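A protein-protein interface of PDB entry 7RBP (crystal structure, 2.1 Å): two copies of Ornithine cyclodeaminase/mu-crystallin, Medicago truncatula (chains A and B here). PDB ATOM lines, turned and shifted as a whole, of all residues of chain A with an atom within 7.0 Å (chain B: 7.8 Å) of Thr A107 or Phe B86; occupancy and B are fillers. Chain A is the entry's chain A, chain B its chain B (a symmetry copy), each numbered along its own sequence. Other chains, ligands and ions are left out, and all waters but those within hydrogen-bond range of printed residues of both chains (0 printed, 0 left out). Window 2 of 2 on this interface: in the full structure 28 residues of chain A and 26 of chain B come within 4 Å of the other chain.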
ATOM      1  N   SER A  70      13.782  25.152 -31.619  1.00  0.00           N
ATOM      2  CA  SER A  70      14.036  23.743 -31.720  1.00  0.00           C
ATOM      3  C   SER A  70      15.463  23.574 -31.268  1.00  0.00           C
ATOM      4  O   SER A  70      16.382  24.150 -31.836  1.00  0.00           O
ATOM      5  CB  SER A  70      13.872  23.251 -33.147  1.00  0.00           C
ATOM      6  OG  SER A  70      14.835  22.276 -33.471  1.00  0.00           O
ATOM      7  N   SER A  71      15.655  22.782 -30.228  1.00  0.00           N
ATOM      8  CA  SER A  71      17.003  22.548 -29.722  1.00  0.00           C
ATOM      9  C   SER A  71      17.482  21.160 -30.136  1.00  0.00           C
ATOM     10  O   SER A  71      18.275  20.536 -29.462  1.00  0.00           O
ATOM     11  CB  SER A  71      17.069  22.750 -28.206  1.00  0.00           C
ATOM     12  OG  SER A  71      17.458  24.070 -27.890  1.00  0.00           O
ATOM     13  N   THR A  72      16.953  20.703 -31.260  1.00  0.00           N
ATOM     14  CA  THR A  72      17.268  19.453 -31.874  1.00  0.00           C
ATOM     15  C   THR A  72      18.150  19.883 -33.002  1.00  0.00           C
ATOM     16  O   THR A  72      17.712  20.551 -33.896  1.00  0.00           O
ATOM     17  CB  THR A  72      16.012  18.844 -32.448  1.00  0.00           C
ATOM     18  OG1 THR A  72      15.278  18.211 -31.405  1.00  0.00           O
ATOM     19  CG2 THR A  72      16.357  17.845 -33.464  1.00  0.00           C
ATOM     20  N   PRO A  73      19.410  19.458 -33.008  1.00  0.00           N
ATOM     21  CA  PRO A  73      20.418  19.852 -33.996  1.00  0.00           C
ATOM     22  C   PRO A  73      20.125  19.593 -35.469  1.00  0.00           C
ATOM     23  O   PRO A  73      20.787  20.197 -36.292  1.00  0.00           O
ATOM     24  CB  PRO A  73      21.651  19.069 -33.566  1.00  0.00           C
ATOM     25  CG  PRO A  73      21.407  18.718 -32.153  1.00  0.00           C
ATOM     26  CD  PRO A  73      19.943  18.473 -32.064  1.00  0.00           C
ATOM     27  N   PRO A  76      18.298  23.360 -36.270  1.00  0.00           N
ATOM     28  CA  PRO A  76      18.849  24.152 -35.151  1.00  0.00           C
ATOM     29  C   PRO A  76      18.556  25.646 -35.247  1.00  0.00           C
ATOM     30  O   PRO A  76      19.445  26.483 -35.453  1.00  0.00           O
ATOM     31  CB  PRO A  76      20.345  23.848 -35.258  1.00  0.00           C
ATOM     32  CG  PRO A  76      20.574  23.683 -36.750  1.00  0.00           C
ATOM     33  CD  PRO A  76      19.266  23.234 -37.377  1.00  0.00           C
ATOM     34  N   TYR A  77      17.292  26.016 -35.052  1.00  0.00           N
ATOM     35  CA  TYR A  77      16.883  27.401 -35.222  1.00  0.00           C
ATOM     36  C   TYR A  77      15.998  27.871 -34.081  1.00  0.00           C
ATOM     37  O   TYR A  77      15.221  27.107 -33.502  1.00  0.00           O
ATOM     38  CB  TYR A  77      16.147  27.606 -36.542  1.00  0.00           C
ATOM     39  CG  TYR A  77      17.059  27.501 -37.729  1.00  0.00           C
ATOM     40  CD1 TYR A  77      17.034  26.386 -38.551  1.00  0.00           C
ATOM     41  CD2 TYR A  77      17.966  28.512 -38.014  1.00  0.00           C
ATOM     42  CE1 TYR A  77      17.877  26.284 -39.632  1.00  0.00           C
ATOM     43  CE2 TYR A  77      18.813  28.419 -39.093  1.00  0.00           C
ATOM     44  CZ  TYR A  77      18.765  27.304 -39.901  1.00  0.00           C
ATOM     45  OH  TYR A  77      19.609  27.209 -40.979  1.00  0.00           O
ATOM     46  N   ILE A  78      16.140  29.156 -33.770  1.00  0.00           N
ATOM     47  CA  ILE A  78      15.209  29.888 -32.924  1.00  0.00           C
ATOM     48  C   ILE A  78      14.646  31.017 -33.771  1.00  0.00           C
ATOM     49  O   ILE A  78      15.359  31.599 -34.592  1.00  0.00           O
ATOM     50  CB  ILE A  78      15.899  30.425 -31.652  1.00  0.00           C
ATOM     51  CG1 ILE A  78      16.643  29.291 -30.950  1.00  0.00           C
ATOM     52  CG2 ILE A  78      14.881  31.056 -30.708  1.00  0.00           C
ATOM     53  CD1 ILE A  78      17.697  29.758 -29.986  1.00  0.00           C
ATOM     54  N   PHE A 104      17.738  32.915 -35.341  1.00  0.00           N
ATOM     55  CA  PHE A 104      18.937  32.681 -34.549  1.00  0.00           C
ATOM     56  C   PHE A 104      19.413  31.245 -34.719  1.00  0.00           C
ATOM     57  O   PHE A 104      18.609  30.322 -34.899  1.00  0.00           O
ATOM     58  CB  PHE A 104      18.735  32.898 -33.031  1.00  0.00           C
ATOM     59  CG  PHE A 104      18.172  34.238 -32.648  1.00  0.00           C
ATOM     60  CD1 PHE A 104      16.866  34.583 -32.952  1.00  0.00           C
ATOM     61  CD2 PHE A 104      18.941  35.134 -31.920  1.00  0.00           C
ATOM     62  CE1 PHE A 104      16.351  35.809 -32.572  1.00  0.00           C
ATOM     63  CE2 PHE A 104      18.427  36.357 -31.534  1.00  0.00           C
ATOM     64  CZ  PHE A 104      17.134  36.698 -31.862  1.00  0.00           C
ATOM     65  N   ASN A 105      20.704  31.040 -34.482  1.00  0.00           N
ATOM     66  CA  ASN A 105      21.322  29.739 -34.505  1.00  0.00           C
ATOM     67  C   ASN A 105      21.013  29.146 -33.175  1.00  0.00           C
ATOM     68  O   ASN A 105      21.381  29.706 -32.196  1.00  0.00           O
ATOM     69  CB  ASN A 105      22.819  29.925 -34.615  1.00  0.00           C
ATOM     70  CG  ASN A 105      23.596  28.638 -34.450  1.00  0.00           C
ATOM     71  OD1 ASN A 105      23.340  27.826 -33.578  1.00  0.00           O
ATOM     72  ND2 ASN A 105      24.566  28.466 -35.296  1.00  0.00           N
ATOM     73  N   SER A 106      20.361  28.006 -33.106  1.00  0.00           N
ATOM     74  CA  SER A 106      20.010  27.475 -31.810  1.00  0.00           C
ATOM     75  C   SER A 106      21.035  26.599 -31.138  1.00  0.00           C
ATOM     76  O   SER A 106      20.769  26.027 -30.105  1.00  0.00           O
ATOM     77  CB  SER A 106      18.694  26.728 -31.883  1.00  0.00           C
ATOM     78  OG  SER A 106      18.880  25.338 -31.982  1.00  0.00           O
ATOM     79  N   THR A 107      22.200  26.471 -31.726  1.00  0.00           N
ATOM     80  CA  THR A 107      23.178  25.623 -31.104  1.00  0.00           C
ATOM     81  C   THR A 107      24.158  26.472 -30.351  1.00  0.00           C
ATOM     82  O   THR A 107      24.632  26.088 -29.310  1.00  0.00           O
ATOM     83  CB  THR A 107      23.867  24.741 -32.128  1.00  0.00           C
ATOM     84  OG1 THR A 107      23.011  23.639 -32.408  1.00  0.00           O
ATOM     85  CG2 THR A 107      25.150  24.225 -31.578  1.00  0.00           C
ATOM     86  N   THR A 108      24.427  27.648 -30.885  1.00  0.00           N
ATOM     87  CA  THR A 108      25.321  28.586 -30.267  1.00  0.00           C
ATOM     88  C   THR A 108      24.592  29.801 -29.713  1.00  0.00           C
ATOM     89  O   THR A 108      25.042  30.418 -28.767  1.00  0.00           O
ATOM     90  CB  THR A 108      26.288  29.107 -31.285  1.00  0.00           C
ATOM     91  OG1 THR A 108      25.583  29.952 -32.179  1.00  0.00           O
ATOM     92  CG2 THR A 108      26.866  27.973 -32.045  1.00  0.00           C
ATOM     93  N   GLY A 109      23.484  30.164 -30.340  1.00  0.00           N
ATOM     94  CA  GLY A 109      22.701  31.297 -29.906  1.00  0.00           C
ATOM     95  C   GLY A 109      22.921  32.597 -30.638  1.00  0.00           C
ATOM     96  O   GLY A 109      22.420  33.606 -30.224  1.00  0.00           O
ATOM     97  N   GLN A 110      23.639  32.582 -31.739  1.00  0.00           N
ATOM     98  CA  GLN A 110      23.894  33.806 -32.477  1.00  0.00           C
ATOM     99  C   GLN A 110      22.744  34.259 -33.380  1.00  0.00           C
ATOM    100  O   GLN A 110      22.038  33.427 -33.888  1.00  0.00           O
ATOM    101  CB  GLN A 110      25.106  33.556 -33.349  1.00  0.00           C
ATOM    102  CG  GLN A 110      25.603  34.734 -34.140  1.00  0.00           C
ATOM    103  CD  GLN A 110      26.295  34.294 -35.401  1.00  0.00           C
ATOM    104  OE1 GLN A 110      26.584  33.113 -35.575  1.00  0.00           O
ATOM    105  NE2 GLN A 110      26.574  35.238 -36.285  1.00  0.00           N
ATOM    106  N   LEU B  57      15.757  27.262 -23.847  1.00  0.00           N
ATOM    107  CA  LEU B  57      15.621  26.544 -25.101  1.00  0.00           C
ATOM    108  C   LEU B  57      16.205  25.151 -25.058  1.00  0.00           C
ATOM    109  O   LEU B  57      15.971  24.374 -25.993  1.00  0.00           O
ATOM    110  CB  LEU B  57      16.332  27.327 -26.196  1.00  0.00           C
ATOM    111  CG  LEU B  57      16.041  28.820 -26.090  1.00  0.00           C
ATOM    112  CD1 LEU B  57      17.050  29.708 -26.818  1.00  0.00           C
ATOM    113  CD2 LEU B  57      14.633  29.106 -26.600  1.00  0.00           C
ATOM    114  N   SER B  58      16.995  24.861 -24.032  1.00  0.00           N
ATOM    115  CA  SER B  58      17.663  23.600 -23.756  1.00  0.00           C
ATOM    116  C   SER B  58      18.177  23.700 -22.325  1.00  0.00           C
ATOM    117  O   SER B  58      18.213  24.807 -21.770  1.00  0.00           O
ATOM    118  CB  SER B  58      18.797  23.342 -24.749  1.00  0.00           C
ATOM    119  OG  SER B  58      19.922  24.138 -24.435  1.00  0.00           O
ATOM    120  N   SER B  60      20.751  24.202 -21.122  1.00  0.00           N
ATOM    121  CA  SER B  60      21.872  25.126 -21.014  1.00  0.00           C
ATOM    122  C   SER B  60      21.643  26.422 -21.790  1.00  0.00           C
ATOM    123  O   SER B  60      22.598  27.169 -22.014  1.00  0.00           O
ATOM    124  CB  SER B  60      23.158  24.448 -21.497  1.00  0.00           C
ATOM    125  OG  SER B  60      24.025  25.379 -22.123  1.00  0.00           O
ATOM    126  N   SER B  61      20.405  26.718 -22.184  1.00  0.00           N
ATOM    127  CA  SER B  61      20.175  27.810 -23.122  1.00  0.00           C
ATOM    128  C   SER B  61      18.892  28.545 -22.779  1.00  0.00           C
ATOM    129  O   SER B  61      17.960  27.957 -22.233  1.00  0.00           O
ATOM    130  CB  SER B  61      20.090  27.284 -24.551  1.00  0.00           C
ATOM    131  OG  SER B  61      18.924  26.495 -24.694  1.00  0.00           O
ATOM    132  N   SER B  62      18.842  29.831 -23.131  1.00  0.00           N
ATOM    133  CA  SER B  62      17.659  30.627 -22.831  1.00  0.00           C
ATOM    134  C   SER B  62      17.508  31.780 -23.808  1.00  0.00           C
ATOM    135  O   SER B  62      18.481  32.269 -24.383  1.00  0.00           O
ATOM    136  CB  SER B  62      17.690  31.193 -21.411  1.00  0.00           C
ATOM    137  OG  SER B  62      18.628  32.228 -21.258  1.00  0.00           O
ATOM    138  N   LEU B  63      16.260  32.227 -23.953  1.00  0.00           N
ATOM    139  CA  LEU B  63      15.896  33.382 -24.763  1.00  0.00           C
ATOM    140  C   LEU B  63      15.087  34.359 -23.919  1.00  0.00           C
ATOM    141  O   LEU B  63      14.235  33.951 -23.122  1.00  0.00           O
ATOM    142  CB  LEU B  63      15.087  32.963 -25.999  1.00  0.00           C
ATOM    143  CG  LEU B  63      14.439  34.089 -26.809  1.00  0.00           C
ATOM    144  CD1 LEU B  63      15.481  34.836 -27.629  1.00  0.00           C
ATOM    145  CD2 LEU B  63      13.330  33.548 -27.700  1.00  0.00           C
ATOM    146  N   VAL B  83      17.463  38.589 -26.617  1.00  0.00           N
ATOM    147  CA  VAL B  83      18.743  38.186 -26.044  1.00  0.00           C
ATOM    148  C   VAL B  83      18.776  36.673 -25.902  1.00  0.00           C
ATOM    149  O   VAL B  83      17.868  36.078 -25.316  1.00  0.00           O
ATOM    150  CB  VAL B  83      18.989  38.852 -24.676  1.00  0.00           C
ATOM    151  CG1 VAL B  83      20.212  38.247 -24.002  1.00  0.00           C
ATOM    152  CG2 VAL B  83      19.149  40.354 -24.828  1.00  0.00           C
ATOM    153  N   THR B  84      19.823  36.051 -26.431  1.00  0.00           N
ATOM    154  CA  THR B  84      20.138  34.659 -26.161  1.00  0.00           C
ATOM    155  C   THR B  84      21.207  34.574 -25.076  1.00  0.00           C
ATOM    156  O   THR B  84      22.186  35.330 -25.091  1.00  0.00           O
ATOM    157  CB  THR B  84      20.630  33.946 -27.422  1.00  0.00           C
ATOM    158  OG1 THR B  84      21.663  34.723 -28.042  1.00  0.00           O
ATOM    159  CG2 THR B  84      19.484  33.750 -28.409  1.00  0.00           C
ATOM    160  N   HIS B  85      20.996  33.653 -24.134  1.00  0.00           N
ATOM    161  CA  HIS B  85      21.954  33.293 -23.093  1.00  0.00           C
ATOM    162  C   HIS B  85      22.367  31.849 -23.339  1.00  0.00           C
ATOM    163  O   HIS B  85      21.553  30.932 -23.175  1.00  0.00           O
ATOM    164  CB  HIS B  85      21.350  33.425 -21.697  1.00  0.00           C
ATOM    165  CG  HIS B  85      21.243  34.829 -21.191  1.00  0.00           C
ATOM    166  ND1 HIS B  85      21.895  35.891 -21.777  1.00  0.00           N
ATOM    167  CD2 HIS B  85      20.556  35.340 -20.141  1.00  0.00           C
ATOM    168  CE1 HIS B  85      21.614  36.997 -21.111  1.00  0.00           C
ATOM    169  NE2 HIS B  85      20.803  36.689 -20.114  1.00  0.00           N
ATOM    170  N   PHE B  86      23.620  31.644 -23.729  1.00  0.00           N
ATOM    171  CA  PHE B  86      24.197  30.311 -23.903  1.00  0.00           C
ATOM    172  C   PHE B  86      25.458  30.232 -23.052  1.00  0.00           C
ATOM    173  O   PHE B  86      26.574  30.289 -23.574  1.00  0.00           O
ATOM    174  CB  PHE B  86      24.511  30.030 -25.374  1.00  0.00           C
ATOM    175  CG  PHE B  86      23.336  29.525 -26.168  1.00  0.00           C
ATOM    176  CD1 PHE B  86      23.384  28.286 -26.786  1.00  0.00           C
ATOM    177  CD2 PHE B  86      22.193  30.296 -26.315  1.00  0.00           C
ATOM    178  CE1 PHE B  86      22.313  27.817 -27.524  1.00  0.00           C
ATOM    179  CE2 PHE B  86      21.117  29.833 -27.051  1.00  0.00           C
ATOM    180  CZ  PHE B  86      21.178  28.592 -27.657  1.00  0.00           C
ATOM    181  N   PRO B  87      25.311  30.099 -21.728  1.00  0.00           N
ATOM    182  CA  PRO B  87      26.496  30.203 -20.852  1.00  0.00           C
ATOM    183  C   PRO B  87      27.606  29.226 -21.200  1.00  0.00           C
ATOM    184  O   PRO B  87      28.785  29.610 -21.208  1.00  0.00           O
ATOM    185  CB  PRO B  87      25.920  29.940 -19.452  1.00  0.00           C
ATOM    186  CG  PRO B  87      24.614  29.249 -19.685  1.00  0.00           C
ATOM    187  CD  PRO B  87      24.085  29.808 -20.969  1.00  0.00           C
ATOM    188  N   GLU B  88      27.265  27.975 -21.519  1.00  0.00           N
ATOM    189  CA  GLU B  88      28.281  26.986 -21.858  1.00  0.00           C
ATOM    190  C   GLU B  88      29.096  27.385 -23.082  1.00  0.00           C
ATOM    191  O   GLU B  88      30.199  26.859 -23.277  1.00  0.00           O
ATOM    192  CB  GLU B  88      27.626  25.621 -22.078  1.00  0.00           C
ATOM    193  CG  GLU B  88      26.911  25.083 -20.845  1.00  0.00           C
ATOM    194  CD  GLU B  88      27.014  23.575 -20.719  1.00  0.00           C
ATOM    195  OE1 GLU B  88      26.069  22.958 -20.182  1.00  0.00           O
ATOM    196  OE2 GLU B  88      28.039  23.011 -21.154  1.00  0.00           O
ATOM    197  N   ASN B  89      28.587  28.314 -23.900  1.00  0.00           N
ATOM    198  CA  ASN B  89      29.370  28.844 -25.014  1.00  0.00           C
ATOM    199  C   ASN B  89      30.725  29.361 -24.549  1.00  0.00           C
ATOM    200  O   ASN B  89      31.714  29.253 -25.282  1.00  0.00           O
ATOM    201  CB  ASN B  89      28.603  29.966 -25.715  1.00  0.00           C
ATOM    202  CG  ASN B  89      27.783  29.473 -26.888  1.00  0.00           C
ATOM    203  OD1 ASN B  89      27.476  28.286 -26.993  1.00  0.00           O
ATOM    204  ND2 ASN B  89      27.427  30.388 -27.783  1.00  0.00           N
ATOM    205  N   SER B  90      30.790  29.914 -23.334  1.00  0.00           N
ATOM    206  CA  SER B  90      32.043  30.461 -22.825  1.00  0.00           C
ATOM    207  C   SER B  90      33.143  29.412 -22.731  1.00  0.00           C
ATOM    208  O   SER B  90      34.320  29.775 -22.620  1.00  0.00           O
ATOM    209  CB  SER B  90      31.819  31.107 -21.458  1.00  0.00           C
ATOM    210  OG  SER B  90      30.570  31.773 -21.406  1.00  0.00           O
ATOM    211  N   SER B  91      32.796  28.126 -22.775  1.00  0.00           N
ATOM    212  CA  SER B  91      33.801  27.072 -22.777  1.00  0.00           C
ATOM    213  C   SER B  91      34.398  26.826 -24.160  1.00  0.00           C
ATOM    214  O   SER B  91      35.032  25.785 -24.367  1.00  0.00           O
ATOM    215  CB  SER B  91      33.202  25.771 -22.232  1.00  0.00           C
ATOM    216  OG  SER B  91      33.846  24.642 -22.793  1.00  0.00           O
ATOM    217  N   LEU B  94      33.099  31.175 -27.595  1.00  0.00           N
ATOM    218  CA  LEU B  94      31.826  31.746 -28.017  1.00  0.00           C
ATOM    219  C   LEU B  94      31.291  32.693 -26.943  1.00  0.00           C
ATOM    220  O   LEU B  94      31.476  32.446 -25.748  1.00  0.00           O
ATOM    221  CB  LEU B  94      30.799  30.645 -28.281  1.00  0.00           C
ATOM    222  CG  LEU B  94      31.082  29.546 -29.303  1.00  0.00           C
ATOM    223  CD1 LEU B  94      29.895  28.593 -29.396  1.00  0.00           C
ATOM    224  CD2 LEU B  94      31.395  30.132 -30.666  1.00  0.00           C
ATOM    225  N   PRO B  95      30.625  33.776 -27.336  1.00  0.00           N
ATOM    226  CA  PRO B  95      30.032  34.678 -26.344  1.00  0.00           C
ATOM    227  C   PRO B  95      28.722  34.125 -25.801  1.00  0.00           C
ATOM    228  O   PRO B  95      27.917  33.540 -26.531  1.00  0.00           O
ATOM    229  CB  PRO B  95      29.805  35.971 -27.137  1.00  0.00           C
ATOM    230  CG  PRO B  95      29.594  35.501 -28.539  1.00  0.00           C
ATOM    231  CD  PRO B  95      30.430  34.257 -28.717  1.00  0.00           C
ATOM    232  N   GLY B  96      28.514  34.319 -24.499  1.00  0.00           N
ATOM    233  CA  GLY B  96      27.331  33.763 -23.860  1.00  0.00           C
ATOM    234  C   GLY B  96      26.073  34.558 -24.166  1.00  0.00           C
ATOM    235  O   GLY B  96      25.016  33.986 -24.448  1.00  0.00           O
ATOM    236  N   VAL B  97      26.173  35.881 -24.119  1.00  0.00           N
ATOM    237  CA  VAL B  97      25.031  36.771 -24.302  1.00  0.00           C
ATOM    238  C   VAL B  97      25.108  37.368 -25.700  1.00  0.00           C
ATOM    239  O   VAL B  97      26.126  37.960 -26.075  1.00  0.00           O
ATOM    240  CB  VAL B  97      25.006  37.868 -23.225  1.00  0.00           C
ATOM    241  CG1 VAL B  97      23.842  38.818 -23.455  1.00  0.00           C
ATOM    242  CG2 VAL B  97      24.943  37.244 -21.839  1.00  0.00           C
ATOM    243  N   GLN B  98      24.042  37.196 -26.480  1.00  0.00           N
ATOM    244  CA  GLN B  98      23.980  37.712 -27.845  1.00  0.00           C
ATOM    245  C   GLN B  98      22.572  38.227 -28.105  1.00  0.00           C
ATOM    246  O   GLN B  98      21.653  37.947 -27.341  1.00  0.00           O
ATOM    247  CB  GLN B  98      24.358  36.634 -28.875  1.00  0.00           C
ATOM    248  CG  GLN B  98      25.710  35.967 -28.633  1.00  0.00           C
ATOM    249  CD  GLN B  98      26.162  35.101 -29.797  1.00  0.00           C
ATOM    250  OE1 GLN B  98      26.752  35.594 -30.759  1.00  0.00           O
ATOM    251  NE2 GLN B  98      25.888  33.804 -29.710  1.00  0.00           N
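The backbone NH (N) of Gln A110 sits close to the side-chain amide nitrogen (NE2) of Gln B98. O of Gly A109 is in hydrogen-bond range of OG1 of Thr B84. The backbone carbonyl oxygen (O) of Thr A108 sits at hydrogen-bond distance from the side-chain amide nitrogen (ND2) of Asn B89. The side-chain hydroxyl (OG) of Ser A71 is in hydrogen-bond range of the backbone carbonyl oxygen (O) of Leu B57 (2.4 Å).
The side-chain hydroxyl (OG1) of Thr A108 sits at hydrogen-bond distance from the backbone NH (N) of Gln A110, at 3.3 Å. The side-chain hydroxyl of Ser B58 is in hydrogen-bond range of the side-chain hydroxyl of Ser B61 (2.6 Å). The backbone carbonyl oxygen (O) of Gln A110 is in hydrogen-bond range of the backbone NH (N) of Asn A105 (2.8 Å). N of Ser A106 lies within hydrogen-bond range of O of Pro A76, 2.9 Å away. The backbone carbonyl oxygen (O) of Ile A78 is in hydrogen-bond range of the backbone NH (N) of Phe A104. The backbone NH (N) of Thr B84 is in hydrogen-bond range of the backbone carbonyl oxygen (O) of Gln B98.
Among the printed residues, merely in contact across the chains: Ser A71 with Ser B58, Ile A78 with Leu B57, Phe A104 with Thr B84, Ser A106 with Phe B86, Thr A107 with Phe B86, Thr A108 with Phe B86, Thr A108 with Gln B98, Gly A109 with Phe B86 and Gly A109 with Gln B98.
Thr A107 touches just one residue of chain B: Phe B86. Ser A106 touches just one residue of chain B: Phe B86. Printed residues of chain B within 4 Å of Phe A104: Thr B84 (3.8 Å). Of the printed residues of chain A, Thr B84 touches Phe A104 and Gly A109. Of the printed residues of chain B, Ile A78 touches Leu B57 (3.2 Å). Of the printed residues of chain B, Thr A108 touches Phe B86 (3.2 Å), Asn B89 (2.6 Å) and Gln B98 (3.6 Å). Printed residues of chain A within 4 Å of Gln B98: Thr A108 (3.6 Å), Gly A109 (3.3 Å) and Gln A110 (3.3 Å). Ser A70 touches none of the printed residues of chain B. The nearest residue of chain B that does not touch Thr A107 is Asn B89 (4.3 Å).
Printed residues of chain B that touch a printed residue of chain A: Leu B57, Ser B58, Thr B84, Phe B86, Asn B89 and Gln B98. Hydrophobic or aromatic side chains of chain B that line the printed part of chain A: Leu B57 and Phe B86. Hydrophobic or aromatic side chains of chain A within 4 Å of the printed part of chain B: Ile A78 and Phe A104.
No position is printed for both chains.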
